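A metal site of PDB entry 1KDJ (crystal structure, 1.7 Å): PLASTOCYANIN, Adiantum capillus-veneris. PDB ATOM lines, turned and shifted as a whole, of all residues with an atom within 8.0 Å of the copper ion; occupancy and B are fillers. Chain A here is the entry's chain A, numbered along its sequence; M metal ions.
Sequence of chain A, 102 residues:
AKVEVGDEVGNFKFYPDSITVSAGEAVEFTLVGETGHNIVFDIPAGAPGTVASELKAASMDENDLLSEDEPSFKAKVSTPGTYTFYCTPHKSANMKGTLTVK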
ATOM      1  N   VAL A   5      13.061 -34.728 -21.395  1.00  0.00           N
ATOM      2  CA  VAL A   5      12.950 -34.013 -20.144  1.00  0.00           C
ATOM      3  C   VAL A   5      14.315 -34.204 -19.457  1.00  0.00           C
ATOM      4  O   VAL A   5      14.617 -35.341 -19.074  1.00  0.00           O
ATOM      5  CB  VAL A   5      11.819 -34.632 -19.309  1.00  0.00           C
ATOM      6  CG1 VAL A   5      11.686 -33.839 -18.014  1.00  0.00           C
ATOM      7  CG2 VAL A   5      10.502 -34.629 -20.083  1.00  0.00           C
ATOM      8  N   GLY A   6      15.071 -33.134 -19.330  1.00  0.00           N
ATOM      9  CA  GLY A   6      16.384 -33.196 -18.685  1.00  0.00           C
ATOM     10  C   GLY A   6      17.411 -33.770 -19.655  1.00  0.00           C
ATOM     11  O   GLY A   6      17.140 -34.111 -20.816  1.00  0.00           O
ATOM     12  N   ASN A  11      20.998 -30.703 -16.336  1.00  0.00           N
ATOM     13  CA  ASN A  11      20.434 -29.385 -16.574  1.00  0.00           C
ATOM     14  C   ASN A  11      18.918 -29.421 -16.396  1.00  0.00           C
ATOM     15  O   ASN A  11      18.297 -30.437 -16.654  1.00  0.00           O
ATOM     16  CB  ASN A  11      20.702 -28.914 -17.976  1.00  0.00           C
ATOM     17  CG  ASN A  11      22.147 -28.559 -18.150  1.00  0.00           C
ATOM     18  OD1 ASN A  11      22.684 -27.701 -17.462  1.00  0.00           O
ATOM     19  ND2 ASN A  11      22.796 -29.176 -19.117  1.00  0.00           N
ATOM     20  N   PHE A  12      18.304 -28.351 -15.968  1.00  0.00           N
ATOM     21  CA  PHE A  12      16.866 -28.347 -15.740  1.00  0.00           C
ATOM     22  C   PHE A  12      16.194 -27.741 -16.996  1.00  0.00           C
ATOM     23  O   PHE A  12      15.786 -26.569 -17.026  1.00  0.00           O
ATOM     24  CB  PHE A  12      16.562 -27.513 -14.517  1.00  0.00           C
ATOM     25  CG  PHE A  12      17.325 -27.880 -13.237  1.00  0.00           C
ATOM     26  CD1 PHE A  12      17.630 -29.198 -12.939  1.00  0.00           C
ATOM     27  CD2 PHE A  12      17.655 -26.845 -12.380  1.00  0.00           C
ATOM     28  CE1 PHE A  12      18.273 -29.479 -11.748  1.00  0.00           C
ATOM     29  CE2 PHE A  12      18.310 -27.136 -11.196  1.00  0.00           C
ATOM     30  CZ  PHE A  12      18.602 -28.453 -10.892  1.00  0.00           C
ATOM     31  N   LYS A  13      16.070 -28.546 -18.055  1.00  0.00           N
ATOM     32  CA  LYS A  13      15.571 -28.047 -19.334  1.00  0.00           C
ATOM     33  C   LYS A  13      14.746 -29.108 -20.007  1.00  0.00           C
ATOM     34  O   LYS A  13      14.969 -30.317 -19.899  1.00  0.00           O
ATOM     35  CB  LYS A  13      16.746 -27.694 -20.267  1.00  0.00           C
ATOM     36  CG  LYS A  13      17.711 -26.557 -19.963  1.00  0.00           C
ATOM     37  CD  LYS A  13      17.236 -25.374 -20.781  1.00  0.00           C
ATOM     38  CE  LYS A  13      18.010 -24.062 -20.586  1.00  0.00           C
ATOM     39  NZ  LYS A  13      17.183 -22.934 -21.072  1.00  0.00           N
ATOM     40  N   PHE A  14      13.777 -28.625 -20.782  1.00  0.00           N
ATOM     41  CA  PHE A  14      13.021 -29.480 -21.688  1.00  0.00           C
ATOM     42  C   PHE A  14      13.691 -29.303 -23.076  1.00  0.00           C
ATOM     43  O   PHE A  14      14.094 -28.191 -23.433  1.00  0.00           O
ATOM     44  CB  PHE A  14      11.532 -29.026 -21.796  1.00  0.00           C
ATOM     45  CG  PHE A  14      10.703 -29.298 -20.534  1.00  0.00           C
ATOM     46  CD1 PHE A  14      10.236 -30.587 -20.336  1.00  0.00           C
ATOM     47  CD2 PHE A  14      10.443 -28.257 -19.643  1.00  0.00           C
ATOM     48  CE1 PHE A  14       9.472 -30.858 -19.199  1.00  0.00           C
ATOM     49  CE2 PHE A  14       9.691 -28.538 -18.513  1.00  0.00           C
ATOM     50  CZ  PHE A  14       9.215 -29.825 -18.319  1.00  0.00           C
ATOM     51  N   LEU A  31      12.083 -39.007 -19.876  1.00  0.00           N
ATOM     52  CA  LEU A  31      13.153 -38.590 -18.988  1.00  0.00           C
ATOM     53  C   LEU A  31      14.523 -38.983 -19.565  1.00  0.00           C
ATOM     54  O   LEU A  31      14.701 -40.112 -20.019  1.00  0.00           O
ATOM     55  CB  LEU A  31      13.004 -39.279 -17.623  1.00  0.00           C
ATOM     56  CG  LEU A  31      14.076 -38.935 -16.622  1.00  0.00           C
ATOM     57  CD1 LEU A  31      13.901 -37.540 -16.105  1.00  0.00           C
ATOM     58  CD2 LEU A  31      14.037 -39.954 -15.520  1.00  0.00           C
ATOM     59  N   THR A  35      18.269 -37.024 -12.809  1.00  0.00           N
ATOM     60  CA  THR A  35      17.447 -36.104 -12.050  1.00  0.00           C
ATOM     61  C   THR A  35      15.949 -36.354 -12.405  1.00  0.00           C
ATOM     62  O   THR A  35      15.606 -36.349 -13.593  1.00  0.00           O
ATOM     63  CB  THR A  35      17.871 -34.695 -12.419  1.00  0.00           C
ATOM     64  OG1 THR A  35      19.282 -34.600 -12.208  1.00  0.00           O
ATOM     65  CG2 THR A  35      17.149 -33.664 -11.625  1.00  0.00           C
ATOM     66  N   GLY A  36      15.066 -36.645 -11.445  1.00  0.00           N
ATOM     67  CA  GLY A  36      13.645 -36.826 -11.681  1.00  0.00           C
ATOM     68  C   GLY A  36      13.051 -35.471 -11.983  1.00  0.00           C
ATOM     69  O   GLY A  36      13.506 -34.379 -11.603  1.00  0.00           O
ATOM     70  N   HIS A  37      11.962 -35.484 -12.757  1.00  0.00           N
ATOM     71  CA  HIS A  37      11.307 -34.258 -13.199  1.00  0.00           C
ATOM     72  C   HIS A  37       9.845 -34.584 -13.393  1.00  0.00           C
ATOM     73  O   HIS A  37       9.495 -35.751 -13.459  1.00  0.00           O
ATOM     74  CB  HIS A  37      11.812 -33.759 -14.569  1.00  0.00           C
ATOM     75  CG  HIS A  37      13.284 -33.349 -14.615  1.00  0.00           C
ATOM     76  ND1 HIS A  37      13.603 -32.149 -14.141  1.00  0.00           N
ATOM     77  CD2 HIS A  37      14.339 -34.017 -15.154  1.00  0.00           C
ATOM     78  CE1 HIS A  37      14.901 -32.044 -14.397  1.00  0.00           C
ATOM     79  NE2 HIS A  37      15.314 -33.143 -14.996  1.00  0.00           N
ATOM     80  N   ASN A  38       8.985 -33.597 -13.535  1.00  0.00           N
ATOM     81  CA  ASN A  38       7.620 -33.945 -13.974  1.00  0.00           C
ATOM     82  C   ASN A  38       7.094 -32.847 -14.901  1.00  0.00           C
ATOM     83  O   ASN A  38       7.829 -31.913 -15.251  1.00  0.00           O
ATOM     84  CB  ASN A  38       6.667 -34.128 -12.758  1.00  0.00           C
ATOM     85  CG  ASN A  38       6.333 -32.890 -11.976  1.00  0.00           C
ATOM     86  OD1 ASN A  38       6.707 -31.742 -12.166  1.00  0.00           O
ATOM     87  ND2 ASN A  38       5.603 -33.142 -10.910  1.00  0.00           N
ATOM     88  N   ILE A  39       5.819 -32.921 -15.291  1.00  0.00           N
ATOM     89  CA  ILE A  39       5.245 -31.956 -16.233  1.00  0.00           C
ATOM     90  C   ILE A  39       3.844 -31.619 -15.720  1.00  0.00           C
ATOM     91  O   ILE A  39       3.035 -32.538 -15.611  1.00  0.00           O
ATOM     92  CB  ILE A  39       5.050 -32.534 -17.683  1.00  0.00           C
ATOM     93  CG1 ILE A  39       6.399 -33.035 -18.270  1.00  0.00           C
ATOM     94  CG2 ILE A  39       4.400 -31.432 -18.578  1.00  0.00           C
ATOM     95  CD1 ILE A  39       6.853 -34.465 -17.886  1.00  0.00           C
ATOM     96  N   LEU A  65       6.973 -38.166 -10.142  1.00  0.00           N
ATOM     97  CA  LEU A  65       8.176 -37.738 -10.834  1.00  0.00           C
ATOM     98  C   LEU A  65       8.471 -38.859 -11.774  1.00  0.00           C
ATOM     99  O   LEU A  65       8.169 -40.014 -11.498  1.00  0.00           O
ATOM    100  CB  LEU A  65       9.396 -37.549  -9.905  1.00  0.00           C
ATOM    101  CG  LEU A  65       9.375 -36.312  -8.996  1.00  0.00           C
ATOM    102  CD1 LEU A  65      10.604 -36.307  -8.138  1.00  0.00           C
ATOM    103  CD2 LEU A  65       9.389 -35.028  -9.782  1.00  0.00           C
ATOM    104  N   TYR A  86       5.433 -26.753 -16.935  1.00  0.00           N
ATOM    105  CA  TYR A  86       6.614 -26.570 -16.101  1.00  0.00           C
ATOM    106  C   TYR A  86       6.887 -27.822 -15.293  1.00  0.00           C
ATOM    107  O   TYR A  86       6.059 -28.743 -15.270  1.00  0.00           O
ATOM    108  CB  TYR A  86       6.406 -25.347 -15.178  1.00  0.00           C
ATOM    109  CG  TYR A  86       5.257 -25.488 -14.187  1.00  0.00           C
ATOM    110  CD1 TYR A  86       5.487 -26.070 -12.950  1.00  0.00           C
ATOM    111  CD2 TYR A  86       3.992 -25.025 -14.536  1.00  0.00           C
ATOM    112  CE1 TYR A  86       4.457 -26.193 -12.047  1.00  0.00           C
ATOM    113  CE2 TYR A  86       2.958 -25.149 -13.624  1.00  0.00           C
ATOM    114  CZ  TYR A  86       3.205 -25.732 -12.401  1.00  0.00           C
ATOM    115  OH  TYR A  86       2.180 -25.877 -11.498  1.00  0.00           O
ATOM    116  N   CYS A  87       8.083 -27.884 -14.711  1.00  0.00           N
ATOM    117  CA  CYS A  87       8.440 -29.011 -13.873  1.00  0.00           C
ATOM    118  C   CYS A  87       8.226 -28.549 -12.442  1.00  0.00           C
ATOM    119  O   CYS A  87       8.822 -27.517 -12.139  1.00  0.00           O
ATOM    120  CB  CYS A  87       9.917 -29.376 -14.080  1.00  0.00           C
ATOM    121  SG  CYS A  87      10.464 -30.591 -12.870  1.00  0.00           S
ATOM    122  N   THR A  88       7.523 -29.218 -11.543  1.00  0.00           N
ATOM    123  CA  THR A  88       7.369 -28.755 -10.173  1.00  0.00           C
ATOM    124  C   THR A  88       8.660 -28.588  -9.347  1.00  0.00           C
ATOM    125  O   THR A  88       8.905 -27.456  -8.946  1.00  0.00           O
ATOM    126  CB  THR A  88       6.387 -29.729  -9.498  1.00  0.00           C
ATOM    127  OG1 THR A  88       5.192 -29.720 -10.295  1.00  0.00           O
ATOM    128  CG2 THR A  88       6.152 -29.374  -8.023  1.00  0.00           C
ATOM    129  N   PRO A  89       9.585 -29.535  -9.150  1.00  0.00           N
ATOM    130  CA  PRO A  89      10.820 -29.315  -8.398  1.00  0.00           C
ATOM    131  C   PRO A  89      11.618 -28.125  -8.910  1.00  0.00           C
ATOM    132  O   PRO A  89      12.104 -27.331  -8.110  1.00  0.00           O
ATOM    133  CB  PRO A  89      11.610 -30.562  -8.525  1.00  0.00           C
ATOM    134  CG  PRO A  89      10.725 -31.642  -8.985  1.00  0.00           C
ATOM    135  CD  PRO A  89       9.573 -30.897  -9.681  1.00  0.00           C
ATOM    136  N   HIS A  90      11.664 -27.927 -10.255  1.00  0.00           N
ATOM    137  CA  HIS A  90      12.619 -26.968 -10.823  1.00  0.00           C
ATOM    138  C   HIS A  90      11.980 -25.749 -11.468  1.00  0.00           C
ATOM    139  O   HIS A  90      12.603 -25.008 -12.241  1.00  0.00           O
ATOM    140  CB  HIS A  90      13.535 -27.726 -11.819  1.00  0.00           C
ATOM    141  CG  HIS A  90      14.255 -28.947 -11.237  1.00  0.00           C
ATOM    142  ND1 HIS A  90      13.933 -30.170 -11.638  1.00  0.00           N
ATOM    143  CD2 HIS A  90      15.252 -28.980 -10.300  1.00  0.00           C
ATOM    144  CE1 HIS A  90      14.696 -31.011 -10.972  1.00  0.00           C
ATOM    145  NE2 HIS A  90      15.471 -30.282 -10.182  1.00  0.00           N
ATOM    146  N   LYS A  91      10.746 -25.478 -11.020  1.00  0.00           N
ATOM    147  CA  LYS A  91       9.953 -24.337 -11.500  1.00  0.00           C
ATOM    148  C   LYS A  91      10.669 -23.027 -11.299  1.00  0.00           C
ATOM    149  O   LYS A  91      10.786 -22.212 -12.202  1.00  0.00           O
ATOM    150  CB  LYS A  91       8.584 -24.248 -10.781  1.00  0.00           C
ATOM    151  CG  LYS A  91       7.600 -23.295 -11.466  1.00  0.00           C
ATOM    152  CD  LYS A  91       6.256 -23.288 -10.722  1.00  0.00           C
ATOM    153  CE  LYS A  91       5.163 -22.490 -11.474  1.00  0.00           C
ATOM    154  NZ  LYS A  91       4.870 -21.210 -10.846  1.00  0.00           N
ATOM    155  N   ALA A  93      13.715 -22.608 -11.202  1.00  0.00           N
ATOM    156  CA  ALA A  93      14.877 -22.583 -12.079  1.00  0.00           C
ATOM    157  C   ALA A  93      14.473 -22.454 -13.555  1.00  0.00           C
ATOM    158  O   ALA A  93      15.235 -22.793 -14.452  1.00  0.00           O
ATOM    159  CB  ALA A  93      15.672 -23.862 -11.866  1.00  0.00           C
ATOM    160  N   MET A  95      12.501 -24.115 -15.511  1.00  0.00           N
ATOM    161  CA  MET A  95      12.317 -25.282 -16.340  1.00  0.00           C
ATOM    162  C   MET A  95      10.810 -25.359 -16.735  1.00  0.00           C
ATOM    163  O   MET A  95       9.909 -25.927 -16.100  1.00  0.00           O
ATOM    164  CB  MET A  95      12.726 -26.535 -15.592  1.00  0.00           C
ATOM    165  CG  MET A  95      12.594 -27.803 -16.365  1.00  0.00           C
ATOM    166  SD  MET A  95      13.318 -29.262 -15.609  1.00  0.00           S
ATOM    167  CE  MET A  95      12.937 -30.486 -16.796  1.00  0.00           C
ATOM    168  N   LYS A  96      10.618 -24.761 -17.921  1.00  0.00           N
ATOM    169  CA  LYS A  96       9.318 -24.579 -18.503  1.00  0.00           C
ATOM    170  C   LYS A  96       9.409 -24.695 -20.028  1.00  0.00           C
ATOM    171  O   LYS A  96      10.502 -24.602 -20.597  1.00  0.00           O
ATOM    172  CB  LYS A  96       8.772 -23.198 -18.087  1.00  0.00           C
ATOM    173  CG  LYS A  96       9.501 -21.971 -18.627  1.00  0.00           C
ATOM    174  CD  LYS A  96       8.735 -20.734 -18.193  1.00  0.00           C
ATOM    175  CE  LYS A  96       9.400 -19.412 -18.630  1.00  0.00           C
ATOM    176  NZ  LYS A  96       9.350 -19.204 -20.060  1.00  0.00           N
HETATM  177 CU    CU M   1      12.684 -30.758 -13.175  1.00  0.00          CU
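The copper ion is bound by ND1 of His 37.
The copper ion is bound by a ring nitrogen (ND1) of His 90, 2.1 Å away.
The copper ion is bound by the side-chain sulfur (SG) of Cys 87, at 2.2 Å.
The copper ion has three donor atoms within binding distance.
Slightly farther from the copper ion lies SD of Met 95 (2.9 Å).
The backbone NH (N) of Met 95 sits at hydrogen-bond distance from the backbone carbonyl oxygen (O) of His 90 (3.4 Å).
SD of Met 95 is in hydrogen-bond range of N of Lys 13, at 3.8 Å.
N of Cys 87 lies within hydrogen-bond range of O of Met 95 (3.0 Å).
The side-chain sulfur (SG) of Cys 87 lies close to the backbone NH (N) of Asn 38 (3.4 Å).
ND1 of His 37 lies close to SD of Met 95, 3.3 Å away.
Of the 22 residues printed, 4 come within 4 Å of the copper ion.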
